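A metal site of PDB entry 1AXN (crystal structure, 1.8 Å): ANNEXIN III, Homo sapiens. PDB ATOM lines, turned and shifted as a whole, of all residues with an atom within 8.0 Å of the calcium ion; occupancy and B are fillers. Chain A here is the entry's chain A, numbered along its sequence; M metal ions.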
ATOM      1  N   GLN A  28      22.166 -26.544 -11.922  1.00  0.00           N
ATOM      2  CA  GLN A  28      23.283 -26.009 -11.139  1.00  0.00           C
ATOM      3  C   GLN A  28      23.539 -24.546 -11.453  1.00  0.00           C
ATOM      4  O   GLN A  28      23.661 -23.748 -10.529  1.00  0.00           O
ATOM      5  CB  GLN A  28      24.514 -26.861 -11.360  1.00  0.00           C
ATOM      6  CG  GLN A  28      25.835 -26.109 -11.137  1.00  0.00           C
ATOM      7  CD  GLN A  28      26.162 -26.074  -9.672  1.00  0.00           C
ATOM      8  OE1 GLN A  28      27.210 -25.569  -9.279  1.00  0.00           O
ATOM      9  NE2 GLN A  28      25.266 -26.615  -8.853  1.00  0.00           N
ATOM     10  N   LYS A  29      23.609 -24.171 -12.715  1.00  0.00           N
ATOM     11  CA  LYS A  29      23.860 -22.783 -13.066  1.00  0.00           C
ATOM     12  C   LYS A  29      22.745 -21.906 -12.501  1.00  0.00           C
ATOM     13  O   LYS A  29      22.958 -20.781 -12.030  1.00  0.00           O
ATOM     14  CB  LYS A  29      24.056 -22.641 -14.567  1.00  0.00           C
ATOM     15  CG  LYS A  29      23.066 -21.942 -15.433  1.00  0.00           C
ATOM     16  CD  LYS A  29      22.007 -22.825 -16.072  1.00  0.00           C
ATOM     17  CE  LYS A  29      20.666 -22.112 -16.137  1.00  0.00           C
ATOM     18  NZ  LYS A  29      19.515 -22.917 -16.564  1.00  0.00           N
ATOM     19  N   ALA A  30      21.512 -22.396 -12.532  1.00  0.00           N
ATOM     20  CA  ALA A  30      20.328 -21.709 -12.063  1.00  0.00           C
ATOM     21  C   ALA A  30      20.313 -21.379 -10.580  1.00  0.00           C
ATOM     22  O   ALA A  30      19.700 -20.358 -10.232  1.00  0.00           O
ATOM     23  CB  ALA A  30      19.088 -22.506 -12.469  1.00  0.00           C
ATOM     24  N   ILE A  31      20.930 -22.171  -9.716  1.00  0.00           N
ATOM     25  CA  ILE A  31      20.867 -21.820  -8.296  1.00  0.00           C
ATOM     26  C   ILE A  31      22.192 -21.283  -7.801  1.00  0.00           C
ATOM     27  O   ILE A  31      22.304 -20.599  -6.789  1.00  0.00           O
ATOM     28  CB  ILE A  31      20.385 -23.014  -7.436  1.00  0.00           C
ATOM     29  CG1 ILE A  31      21.453 -24.094  -7.351  1.00  0.00           C
ATOM     30  CG2 ILE A  31      19.081 -23.583  -7.961  1.00  0.00           C
ATOM     31  CD1 ILE A  31      21.014 -25.371  -6.700  1.00  0.00           C
ATOM     32  N   ARG A  32      23.246 -21.612  -8.538  1.00  0.00           N
ATOM     33  CA  ARG A  32      24.592 -21.193  -8.195  1.00  0.00           C
ATOM     34  C   ARG A  32      24.721 -19.688  -8.024  1.00  0.00           C
ATOM     35  O   ARG A  32      24.239 -18.886  -8.837  1.00  0.00           O
ATOM     36  CB  ARG A  32      25.480 -21.692  -9.332  1.00  0.00           C
ATOM     37  CG  ARG A  32      26.901 -22.058  -8.953  1.00  0.00           C
ATOM     38  CD  ARG A  32      27.760 -21.272  -9.909  1.00  0.00           C
ATOM     39  NE  ARG A  32      28.395 -21.856 -11.039  1.00  0.00           N
ATOM     40  CZ  ARG A  32      28.918 -23.024 -11.318  1.00  0.00           C
ATOM     41  NH1 ARG A  32      28.902 -24.042 -10.468  1.00  0.00           N
ATOM     42  NH2 ARG A  32      29.465 -23.199 -12.514  1.00  0.00           N
ATOM     43  N   GLY A  33      25.381 -19.270  -6.941  1.00  0.00           N
ATOM     44  CA  GLY A  33      25.589 -17.864  -6.666  1.00  0.00           C
ATOM     45  C   GLY A  33      24.467 -17.072  -6.047  1.00  0.00           C
ATOM     46  O   GLY A  33      23.590 -17.627  -5.388  1.00  0.00           O
ATOM     47  N   ILE A  34      24.484 -15.748  -6.253  1.00  0.00           N
ATOM     48  CA  ILE A  34      23.436 -14.922  -5.665  1.00  0.00           C
ATOM     49  C   ILE A  34      22.205 -15.030  -6.559  1.00  0.00           C
ATOM     50  O   ILE A  34      22.295 -14.993  -7.775  1.00  0.00           O
ATOM     51  CB  ILE A  34      23.762 -13.431  -5.445  1.00  0.00           C
ATOM     52  CG1 ILE A  34      24.642 -13.172  -4.215  1.00  0.00           C
ATOM     53  CG2 ILE A  34      22.496 -12.569  -5.280  1.00  0.00           C
ATOM     54  CD1 ILE A  34      24.960 -11.702  -3.998  1.00  0.00           C
ATOM     55  N   GLY A  35      21.072 -15.155  -5.893  1.00  0.00           N
ATOM     56  CA  GLY A  35      19.821 -15.240  -6.626  1.00  0.00           C
ATOM     57  C   GLY A  35      19.623 -16.688  -7.076  1.00  0.00           C
ATOM     58  O   GLY A  35      20.396 -17.601  -6.800  1.00  0.00           O
ATOM     59  N   THR A  36      18.516 -16.785  -7.795  1.00  0.00           N
ATOM     60  CA  THR A  36      18.104 -18.071  -8.311  1.00  0.00           C
ATOM     61  C   THR A  36      17.305 -17.873  -9.574  1.00  0.00           C
ATOM     62  O   THR A  36      16.515 -16.919  -9.633  1.00  0.00           O
ATOM     63  CB  THR A  36      17.189 -18.714  -7.235  1.00  0.00           C
ATOM     64  OG1 THR A  36      17.943 -18.710  -6.016  1.00  0.00           O
ATOM     65  CG2 THR A  36      16.766 -20.107  -7.650  1.00  0.00           C
ATOM     66  N   ASP A  37      17.529 -18.744 -10.549  1.00  0.00           N
ATOM     67  CA  ASP A  37      16.730 -18.606 -11.773  1.00  0.00           C
ATOM     68  C   ASP A  37      15.549 -19.568 -11.521  1.00  0.00           C
ATOM     69  O   ASP A  37      15.590 -20.705 -11.980  1.00  0.00           O
ATOM     70  CB  ASP A  37      17.507 -18.912 -13.032  1.00  0.00           C
ATOM     71  CG  ASP A  37      16.756 -18.611 -14.318  1.00  0.00           C
ATOM     72  OD1 ASP A  37      15.561 -18.257 -14.292  1.00  0.00           O
ATOM     73  OD2 ASP A  37      17.375 -18.713 -15.403  1.00  0.00           O
ATOM     74  N   ASP A  71      20.146 -28.478  -2.237  1.00  0.00           N
ATOM     75  CA  ASP A  71      20.382 -27.181  -2.873  1.00  0.00           C
ATOM     76  C   ASP A  71      19.061 -26.451  -3.050  1.00  0.00           C
ATOM     77  O   ASP A  71      18.966 -25.236  -2.909  1.00  0.00           O
ATOM     78  CB  ASP A  71      21.088 -27.342  -4.206  1.00  0.00           C
ATOM     79  CG  ASP A  71      22.586 -27.425  -3.999  1.00  0.00           C
ATOM     80  OD1 ASP A  71      23.034 -27.340  -2.844  1.00  0.00           O
ATOM     81  OD2 ASP A  71      23.300 -27.590  -4.994  1.00  0.00           O
ATOM     82  N   GLY A  74      18.044 -24.911   0.201  1.00  0.00           N
ATOM     83  CA  GLY A  74      18.872 -23.769   0.560  1.00  0.00           C
ATOM     84  C   GLY A  74      18.566 -22.498  -0.211  1.00  0.00           C
ATOM     85  O   GLY A  74      18.743 -21.393   0.290  1.00  0.00           O
ATOM     86  N   ASP A  75      18.087 -22.639  -1.447  1.00  0.00           N
ATOM     87  CA  ASP A  75      17.770 -21.515  -2.300  1.00  0.00           C
ATOM     88  C   ASP A  75      16.327 -21.095  -2.388  1.00  0.00           C
ATOM     89  O   ASP A  75      16.078 -19.912  -2.567  1.00  0.00           O
ATOM     90  CB  ASP A  75      18.105 -21.904  -3.768  1.00  0.00           C
ATOM     91  CG  ASP A  75      19.353 -21.232  -4.306  1.00  0.00           C
ATOM     92  OD1 ASP A  75      20.402 -21.286  -3.624  1.00  0.00           O
ATOM     93  OD2 ASP A  75      19.284 -20.655  -5.418  1.00  0.00           O
ATOM     94  N   LEU A  76      15.440 -22.089  -2.287  1.00  0.00           N
ATOM     95  CA  LEU A  76      14.028 -21.785  -2.393  1.00  0.00           C
ATOM     96  C   LEU A  76      13.346 -21.630  -1.023  1.00  0.00           C
ATOM     97  O   LEU A  76      13.880 -22.134  -0.057  1.00  0.00           O
ATOM     98  CB  LEU A  76      13.338 -22.871  -3.217  1.00  0.00           C
ATOM     99  CG  LEU A  76      13.947 -23.197  -4.586  1.00  0.00           C
ATOM    100  CD1 LEU A  76      12.997 -24.086  -5.382  1.00  0.00           C
ATOM    101  CD2 LEU A  76      14.265 -21.921  -5.369  1.00  0.00           C
HETATM  102 CA    CA M   1      21.417 -18.985  -5.439  1.00  0.00          CA
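The side-chain carboxylate (OD2) of Asp 75 lies close to the side-chain hydroxyl (OG1) of Thr 36 (2.4 Å).
Residues that only touch the calcium ion: Thr 36 (3.5 Å). The nearest printed residue that does not touch the calcium ion is Ile 34 (4.2 Å).
The calcium ion is bound by the backbone carbonyl oxygen of Gly 35 (2.2 Å), the backbone carbonyl oxygen of Ile 31 (2.3 Å), the backbone carbonyl oxygen of Gly 33 (2.6 Å) and the side-chain carboxylate of Asp 75 (2.7 Å). The calcium ion has four donor atoms within binding distance. Slightly farther from the calcium ion lies the side-chain carboxylate (OD1) of Asp 75 (3.1 Å).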
